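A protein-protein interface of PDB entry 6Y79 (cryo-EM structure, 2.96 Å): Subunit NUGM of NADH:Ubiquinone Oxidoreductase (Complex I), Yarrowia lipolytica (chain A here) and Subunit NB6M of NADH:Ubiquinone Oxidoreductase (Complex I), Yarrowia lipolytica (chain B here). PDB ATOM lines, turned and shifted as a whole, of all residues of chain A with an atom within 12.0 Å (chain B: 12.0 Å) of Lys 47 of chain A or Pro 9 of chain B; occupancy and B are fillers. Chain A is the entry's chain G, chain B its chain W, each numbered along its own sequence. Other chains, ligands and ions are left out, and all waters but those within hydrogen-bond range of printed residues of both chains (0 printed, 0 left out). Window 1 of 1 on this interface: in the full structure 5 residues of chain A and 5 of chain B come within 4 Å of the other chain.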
ATOM      1  N   LYS A  40     -38.167  34.114 -20.524  1.00  0.00           N
ATOM      2  CA  LYS A  40     -36.951  33.399 -20.856  1.00  0.00           C
ATOM      3  C   LYS A  40     -37.104  31.914 -20.551  1.00  0.00           C
ATOM      4  O   LYS A  40     -37.826  31.510 -19.637  1.00  0.00           O
ATOM      5  CB  LYS A  40     -35.757  33.977 -20.095  1.00  0.00           C
ATOM      6  CG  LYS A  40     -35.877  33.907 -18.587  1.00  0.00           C
ATOM      7  CD  LYS A  40     -34.688  34.555 -17.905  1.00  0.00           C
ATOM      8  CE  LYS A  40     -33.413  33.767 -18.157  1.00  0.00           C
ATOM      9  NZ  LYS A  40     -33.447  32.418 -17.535  1.00  0.00           N
ATOM     10  N   ASP A  41     -36.437  31.101 -21.357  1.00  0.00           N
ATOM     11  CA  ASP A  41     -36.256  29.694 -21.059  1.00  0.00           C
ATOM     12  C   ASP A  41     -35.104  29.533 -20.085  1.00  0.00           C
ATOM     13  O   ASP A  41     -34.182  30.353 -20.043  1.00  0.00           O
ATOM     14  CB  ASP A  41     -35.971  28.907 -22.330  1.00  0.00           C
ATOM     15  CG  ASP A  41     -36.473  27.501 -22.255  1.00  0.00           C
ATOM     16  OD1 ASP A  41     -36.910  27.083 -21.160  1.00  0.00           O
ATOM     17  OD2 ASP A  41     -36.442  26.806 -23.294  1.00  0.00           O
ATOM     18  N   ILE A  42     -35.149  28.460 -19.303  1.00  0.00           N
ATOM     19  CA  ILE A  42     -34.028  28.180 -18.417  1.00  0.00           C
ATOM     20  C   ILE A  42     -33.264  26.937 -18.847  1.00  0.00           C
ATOM     21  O   ILE A  42     -32.218  26.631 -18.270  1.00  0.00           O
ATOM     22  CB  ILE A  42     -34.499  28.059 -16.963  1.00  0.00           C
ATOM     23  CG1 ILE A  42     -35.540  26.955 -16.836  1.00  0.00           C
ATOM     24  CG2 ILE A  42     -35.062  29.371 -16.465  1.00  0.00           C
ATOM     25  CD1 ILE A  42     -35.951  26.732 -15.421  1.00  0.00           C
ATOM     26  N   ARG A  43     -33.776  26.199 -19.831  1.00  0.00           N
ATOM     27  CA  ARG A  43     -33.022  25.081 -20.384  1.00  0.00           C
ATOM     28  C   ARG A  43     -31.784  25.560 -21.134  1.00  0.00           C
ATOM     29  O   ARG A  43     -30.759  24.872 -21.134  1.00  0.00           O
ATOM     30  CB  ARG A  43     -33.921  24.256 -21.295  1.00  0.00           C
ATOM     31  CG  ARG A  43     -35.276  23.999 -20.688  1.00  0.00           C
ATOM     32  CD  ARG A  43     -36.179  23.265 -21.651  1.00  0.00           C
ATOM     33  NE  ARG A  43     -36.701  24.151 -22.680  1.00  0.00           N
ATOM     34  CZ  ARG A  43     -37.026  23.763 -23.905  1.00  0.00           C
ATOM     35  NH1 ARG A  43     -37.494  24.643 -24.773  1.00  0.00           N
ATOM     36  NH2 ARG A  43     -36.873  22.503 -24.267  1.00  0.00           N
ATOM     37  N   LEU A  44     -31.857  26.731 -21.768  1.00  0.00           N
ATOM     38  CA  LEU A  44     -30.702  27.387 -22.378  1.00  0.00           C
ATOM     39  C   LEU A  44     -30.090  28.290 -21.326  1.00  0.00           C
ATOM     40  O   LEU A  44     -30.551  29.414 -21.106  1.00  0.00           O
ATOM     41  CB  LEU A  44     -31.091  28.198 -23.606  1.00  0.00           C
ATOM     42  CG  LEU A  44     -31.594  27.552 -24.890  1.00  0.00           C
ATOM     43  CD1 LEU A  44     -32.009  28.661 -25.838  1.00  0.00           C
ATOM     44  CD2 LEU A  44     -30.549  26.642 -25.537  1.00  0.00           C
ATOM     45  N   ASP A  45     -29.034  27.802 -20.700  1.00  0.00           N
ATOM     46  CA  ASP A  45     -28.465  28.464 -19.538  1.00  0.00           C
ATOM     47  C   ASP A  45     -27.043  27.952 -19.390  1.00  0.00           C
ATOM     48  O   ASP A  45     -26.709  26.900 -19.938  1.00  0.00           O
ATOM     49  CB  ASP A  45     -29.334  28.169 -18.299  1.00  0.00           C
ATOM     50  CG  ASP A  45     -28.795  28.757 -17.015  1.00  0.00           C
ATOM     51  OD1 ASP A  45     -28.951  29.963 -16.772  1.00  0.00           O
ATOM     52  OD2 ASP A  45     -28.240  27.948 -16.273  1.00  0.00           O
ATOM     53  N   PRO A  46     -26.148  28.728 -18.767  1.00  0.00           N
ATOM     54  CA  PRO A  46     -24.857  28.138 -18.375  1.00  0.00           C
ATOM     55  C   PRO A  46     -25.037  27.417 -17.053  1.00  0.00           C
ATOM     56  O   PRO A  46     -25.417  28.018 -16.056  1.00  0.00           O
ATOM     57  CB  PRO A  46     -23.930  29.355 -18.247  1.00  0.00           C
ATOM     58  CG  PRO A  46     -24.579  30.399 -19.088  1.00  0.00           C
ATOM     59  CD  PRO A  46     -26.050  30.186 -18.893  1.00  0.00           C
ATOM     60  N   LYS A  47     -24.792  26.126 -17.035  1.00  0.00           N
ATOM     61  CA  LYS A  47     -25.052  25.406 -15.801  1.00  0.00           C
ATOM     62  C   LYS A  47     -23.763  25.176 -15.030  1.00  0.00           C
ATOM     63  O   LYS A  47     -22.662  25.434 -15.526  1.00  0.00           O
ATOM     64  CB  LYS A  47     -25.772  24.080 -16.058  1.00  0.00           C
ATOM     65  CG  LYS A  47     -27.192  24.298 -16.554  1.00  0.00           C
ATOM     66  CD  LYS A  47     -27.916  22.994 -16.816  1.00  0.00           C
ATOM     67  CE  LYS A  47     -29.338  23.251 -17.277  1.00  0.00           C
ATOM     68  NZ  LYS A  47     -30.079  24.086 -16.297  1.00  0.00           N
ATOM     69  N   VAL A  48     -23.929  24.750 -13.776  1.00  0.00           N
ATOM     70  CA  VAL A  48     -22.794  24.335 -12.965  1.00  0.00           C
ATOM     71  C   VAL A  48     -22.132  23.133 -13.615  1.00  0.00           C
ATOM     72  O   VAL A  48     -22.811  22.239 -14.157  1.00  0.00           O
ATOM     73  CB  VAL A  48     -23.220  23.969 -11.534  1.00  0.00           C
ATOM     74  CG1 VAL A  48     -21.997  23.768 -10.641  1.00  0.00           C
ATOM     75  CG2 VAL A  48     -24.097  25.024 -10.951  1.00  0.00           C
ATOM     76  N   HIS A  49     -20.798  23.121 -13.574  1.00  0.00           N
ATOM     77  CA  HIS A  49     -20.031  21.981 -14.024  1.00  0.00           C
ATOM     78  C   HIS A  49     -18.746  21.895 -13.230  1.00  0.00           C
ATOM     79  O   HIS A  49     -17.953  22.833 -13.243  1.00  0.00           O
ATOM     80  CB  HIS A  49     -19.746  22.092 -15.502  1.00  0.00           C
ATOM     81  CG  HIS A  49     -18.953  20.953 -16.030  1.00  0.00           C
ATOM     82  ND1 HIS A  49     -17.982  21.099 -16.995  1.00  0.00           N
ATOM     83  CD2 HIS A  49     -18.987  19.638 -15.722  1.00  0.00           C
ATOM     84  CE1 HIS A  49     -17.458  19.917 -17.264  1.00  0.00           C
ATOM     85  NE2 HIS A  49     -18.052  19.014 -16.507  1.00  0.00           N
ATOM     86  N   VAL A  50     -18.527  20.751 -12.603  1.00  0.00           N
ATOM     87  CA  VAL A  50     -17.308  20.436 -11.872  1.00  0.00           C
ATOM     88  C   VAL A  50     -16.427  19.551 -12.739  1.00  0.00           C
ATOM     89  O   VAL A  50     -16.902  18.759 -13.557  1.00  0.00           O
ATOM     90  CB  VAL A  50     -17.623  19.749 -10.523  1.00  0.00           C
ATOM     91  CG1 VAL A  50     -18.382  20.690  -9.603  1.00  0.00           C
ATOM     92  CG2 VAL A  50     -18.421  18.467 -10.731  1.00  0.00           C
ATOM     93  N   ASP A  51     -15.120  19.689 -12.574  1.00  0.00           N
ATOM     94  CA  ASP A  51     -14.231  18.706 -13.173  1.00  0.00           C
ATOM     95  C   ASP A  51     -14.285  17.390 -12.421  1.00  0.00           C
ATOM     96  O   ASP A  51     -14.230  16.327 -13.048  1.00  0.00           O
ATOM     97  CB  ASP A  51     -12.783  19.216 -13.188  1.00  0.00           C
ATOM     98  CG  ASP A  51     -12.263  19.523 -11.801  1.00  0.00           C
ATOM     99  OD1 ASP A  51     -13.085  19.926 -10.951  1.00  0.00           O
ATOM    100  OD2 ASP A  51     -11.053  19.334 -11.547  1.00  0.00           O
ATOM    101  N   VAL A  53     -15.357  15.769  -8.157  1.00  0.00           N
ATOM    102  CA  VAL A  53     -15.990  15.985  -6.865  1.00  0.00           C
ATOM    103  C   VAL A  53     -15.007  15.578  -5.776  1.00  0.00           C
ATOM    104  O   VAL A  53     -14.282  14.589  -5.927  1.00  0.00           O
ATOM    105  CB  VAL A  53     -17.308  15.190  -6.788  1.00  0.00           C
ATOM    106  CG1 VAL A  53     -18.032  15.408  -5.466  1.00  0.00           C
ATOM    107  CG2 VAL A  53     -18.189  15.574  -7.958  1.00  0.00           C
ATOM    108  N   SER B   3     -17.855  13.446 -12.653  1.00  0.00           N
ATOM    109  CA  SER B   3     -19.247  13.787 -12.908  1.00  0.00           C
ATOM    110  C   SER B   3     -19.391  14.304 -14.332  1.00  0.00           C
ATOM    111  O   SER B   3     -18.887  15.384 -14.652  1.00  0.00           O
ATOM    112  CB  SER B   3     -19.739  14.834 -11.905  1.00  0.00           C
ATOM    113  OG  SER B   3     -21.067  15.231 -12.187  1.00  0.00           O
ATOM    114  N   VAL B   4     -20.057  13.519 -15.193  1.00  0.00           N
ATOM    115  CA  VAL B   4     -20.375  13.914 -16.567  1.00  0.00           C
ATOM    116  C   VAL B   4     -21.825  13.556 -16.879  1.00  0.00           C
ATOM    117  O   VAL B   4     -22.236  12.401 -16.722  1.00  0.00           O
ATOM    118  CB  VAL B   4     -19.458  13.249 -17.619  1.00  0.00           C
ATOM    119  CG1 VAL B   4     -19.687  13.892 -18.977  1.00  0.00           C
ATOM    120  CG2 VAL B   4     -17.972  13.314 -17.264  1.00  0.00           C
ATOM    121  N   GLY B   5     -22.605  14.528 -17.344  1.00  0.00           N
ATOM    122  CA  GLY B   5     -23.927  14.255 -17.876  1.00  0.00           C
ATOM    123  C   GLY B   5     -25.057  14.283 -16.876  1.00  0.00           C
ATOM    124  O   GLY B   5     -26.159  13.820 -17.198  1.00  0.00           O
ATOM    125  N   GLN B   6     -24.830  14.807 -15.681  1.00  0.00           N
ATOM    126  CA  GLN B   6     -25.870  14.865 -14.670  1.00  0.00           C
ATOM    127  C   GLN B   6     -26.724  16.111 -14.832  1.00  0.00           C
ATOM    128  O   GLN B   6     -26.371  17.054 -15.541  1.00  0.00           O
ATOM    129  CB  GLN B   6     -25.278  14.884 -13.271  1.00  0.00           C
ATOM    130  CG  GLN B   6     -24.659  13.631 -12.779  1.00  0.00           C
ATOM    131  CD  GLN B   6     -24.178  13.831 -11.377  1.00  0.00           C
ATOM    132  OE1 GLN B   6     -23.846  14.944 -10.988  1.00  0.00           O
ATOM    133  NE2 GLN B   6     -24.180  12.777 -10.593  1.00  0.00           N
ATOM    134  N   ASP B   7     -27.861  16.099 -14.146  1.00  0.00           N
ATOM    135  CA  ASP B   7     -28.650  17.301 -13.936  1.00  0.00           C
ATOM    136  C   ASP B   7     -27.993  18.120 -12.835  1.00  0.00           C
ATOM    137  O   ASP B   7     -27.758  17.622 -11.735  1.00  0.00           O
ATOM    138  CB  ASP B   7     -30.083  16.927 -13.555  1.00  0.00           C
ATOM    139  CG  ASP B   7     -31.052  18.091 -13.629  1.00  0.00           C
ATOM    140  OD1 ASP B   7     -30.641  19.237 -13.922  1.00  0.00           O
ATOM    141  OD2 ASP B   7     -32.252  17.844 -13.408  1.00  0.00           O
ATOM    142  N   LEU B   8     -27.684  19.367 -13.141  1.00  0.00           N
ATOM    143  CA  LEU B   8     -27.034  20.313 -12.250  1.00  0.00           C
ATOM    144  C   LEU B   8     -27.847  21.596 -12.256  1.00  0.00           C
ATOM    145  O   LEU B   8     -28.620  21.840 -13.187  1.00  0.00           O
ATOM    146  CB  LEU B   8     -25.593  20.621 -12.695  1.00  0.00           C
ATOM    147  CG  LEU B   8     -24.389  19.771 -12.290  1.00  0.00           C
ATOM    148  CD1 LEU B   8     -24.273  19.680 -10.788  1.00  0.00           C
ATOM    149  CD2 LEU B   8     -24.429  18.415 -12.919  1.00  0.00           C
ATOM    150  N   PRO B   9     -27.713  22.430 -11.227  1.00  0.00           N
ATOM    151  CA  PRO B   9     -28.379  23.742 -11.238  1.00  0.00           C
ATOM    152  C   PRO B   9     -27.698  24.738 -12.167  1.00  0.00           C
ATOM    153  O   PRO B   9     -26.714  24.405 -12.838  1.00  0.00           O
ATOM    154  CB  PRO B   9     -28.278  24.180  -9.768  1.00  0.00           C
ATOM    155  CG  PRO B   9     -27.122  23.457  -9.249  1.00  0.00           C
ATOM    156  CD  PRO B   9     -27.225  22.112  -9.875  1.00  0.00           C
ATOM    157  N   PRO B  10     -28.267  25.941 -12.318  1.00  0.00           N
ATOM    158  CA  PRO B  10     -27.609  27.035 -13.059  1.00  0.00           C
ATOM    159  C   PRO B  10     -26.340  27.615 -12.437  1.00  0.00           C
ATOM    160  O   PRO B  10     -26.125  27.528 -11.224  1.00  0.00           O
ATOM    161  CB  PRO B  10     -28.701  28.103 -13.088  1.00  0.00           C
ATOM    162  CG  PRO B  10     -29.934  27.330 -13.185  1.00  0.00           C
ATOM    163  CD  PRO B  10     -29.735  26.066 -12.403  1.00  0.00           C
ATOM    164  N   VAL B  11     -25.559  28.320 -13.286  1.00  0.00           N
ATOM    165  CA  VAL B  11     -24.310  28.975 -12.872  1.00  0.00           C
ATOM    166  C   VAL B  11     -24.587  30.021 -11.801  1.00  0.00           C
ATOM    167  O   VAL B  11     -23.780  30.199 -10.883  1.00  0.00           O
ATOM    168  CB  VAL B  11     -23.539  29.619 -14.059  1.00  0.00           C
ATOM    169  CG1 VAL B  11     -24.272  30.799 -14.742  1.00  0.00           C
ATOM    170  CG2 VAL B  11     -22.091  30.028 -13.658  1.00  0.00           C
ATOM    171  N   GLY B  12     -25.743  30.689 -11.853  1.00  0.00           N
ATOM    172  CA  GLY B  12     -26.081  31.704 -10.874  1.00  0.00           C
ATOM    173  C   GLY B  12     -27.270  31.369 -10.040  1.00  0.00           C
ATOM    174  O   GLY B  12     -27.706  32.185  -9.224  1.00  0.00           O
ATOM    175  N   GLY B  13     -27.825  30.187 -10.259  1.00  0.00           N
ATOM    176  CA  GLY B  13     -29.012  29.754  -9.568  1.00  0.00           C
ATOM    177  C   GLY B  13     -30.268  30.285 -10.221  1.00  0.00           C
ATOM    178  O   GLY B  13     -30.247  31.122 -11.125  1.00  0.00           O
ATOM    179  N   TYR B  14     -31.387  29.760  -9.754  1.00  0.00           N
ATOM    180  CA  TYR B  14     -32.680  30.272 -10.149  1.00  0.00           C
ATOM    181  C   TYR B  14     -33.005  31.529  -9.349  1.00  0.00           C
ATOM    182  O   TYR B  14     -32.448  31.771  -8.277  1.00  0.00           O
ATOM    183  CB  TYR B  14     -33.748  29.215  -9.918  1.00  0.00           C
ATOM    184  CG  TYR B  14     -33.513  27.895 -10.611  1.00  0.00           C
ATOM    185  CD1 TYR B  14     -33.829  27.732 -11.948  1.00  0.00           C
ATOM    186  CD2 TYR B  14     -33.011  26.803  -9.916  1.00  0.00           C
ATOM    187  CE1 TYR B  14     -33.635  26.525 -12.582  1.00  0.00           C
ATOM    188  CE2 TYR B  14     -32.811  25.592 -10.542  1.00  0.00           C
ATOM    189  CZ  TYR B  14     -33.129  25.460 -11.874  1.00  0.00           C
ATOM    190  OH  TYR B  14     -32.925  24.260 -12.504  1.00  0.00           O
ATOM    191  N   GLU B  15     -33.910  32.342  -9.886  1.00  0.00           N
ATOM    192  CA  GLU B  15     -34.357  33.523  -9.167  1.00  0.00           C
ATOM    193  C   GLU B  15     -35.462  33.120  -8.182  1.00  0.00           C
ATOM    194  O   GLU B  15     -36.093  32.079  -8.360  1.00  0.00           O
ATOM    195  CB  GLU B  15     -34.814  34.596 -10.162  1.00  0.00           C
ATOM    196  CG  GLU B  15     -35.771  34.145 -11.222  1.00  0.00           C
ATOM    197  CD  GLU B  15     -36.435  35.307 -11.924  1.00  0.00           C
ATOM    198  OE1 GLU B  15     -35.711  36.147 -12.494  1.00  0.00           O
ATOM    199  OE2 GLU B  15     -37.679  35.387 -11.897  1.00  0.00           O
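Asp 41 of chain A touches none of the printed residues of chain B.
Of chain B, only Pro 10 (3.2 Å) comes within 4 Å of Asp 45 of chain A.
Pro 46 of chain A touches two residues of chain B.
Of the printed residues of chain B, Lys 47 of chain A touches Leu 8, Pro 9 and Val 11.
Val 48 of chain A touches four residues of chain B.
Val 50 of chain A touches none of the printed residues of chain B.
No residue of chain A comes within 4 Å of Asp 7 of chain B.
Leu 8 of chain B touches two residues of chain A.
Pro 9 of chain B touches two residues of chain A.
Pro 10 of chain B touches just these residues of chain A: Asp 45 (3.2 Å), Pro 46 (3.8 Å) and Val 48 (3.2 Å).
Of the printed residues of chain A, Val 11 of chain B touches Pro 46 (2.8 Å), Lys 47 (3.9 Å) and Val 48 (3.95 Å).
Printed residues of chain A within 4 Å of Tyr 14 of chain B: Ile 42 (3.7 Å).
Tyr 14 of chain B touches Ile 42 of chain A.
Asp 45 of chain A touches Pro 10 of chain B (OD2 to CB, 3.2 Å).
Pro 46 of chain A touches Pro 10 of chain B (O to C, 3.8 Å).
O of Leu 8 of chain B touches CD of Lys 47 of chain A, 3.9 Å away.
Pro 9 of chain B touches Lys 47 of chain A.
N of Val 11 of chain B touches CA of Lys 47 of chain A (3.9 Å).
Val 48 of chain A touches Leu 8 of chain B.
CG2 of Val 48 of chain A touches O of Pro 10 of chain B (3.2 Å).
Val 48 of chain A touches Val 11 of chain B (N to N, 3.95 Å).
Of the 13 printed residues of chain B, 5 touch a printed residue of chain A.
Among the printed residues, 11 pairs touch across the chains.
Among the printed residues, no Asp or Glu carboxylate lies within 4 Å of a Lys or Arg side-chain nitrogen of the other chain.
The backbone NH (N) of Val 11 of chain B sits at hydrogen-bond distance from the backbone carbonyl oxygen (O) of Pro 46 of chain A, 2.8 Å away.
The backbone carbonyl oxygen (O) of Pro 9 of chain B is in hydrogen-bond range of the backbone NH (N) of Val 48 of chain A, at 3.0 Å.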
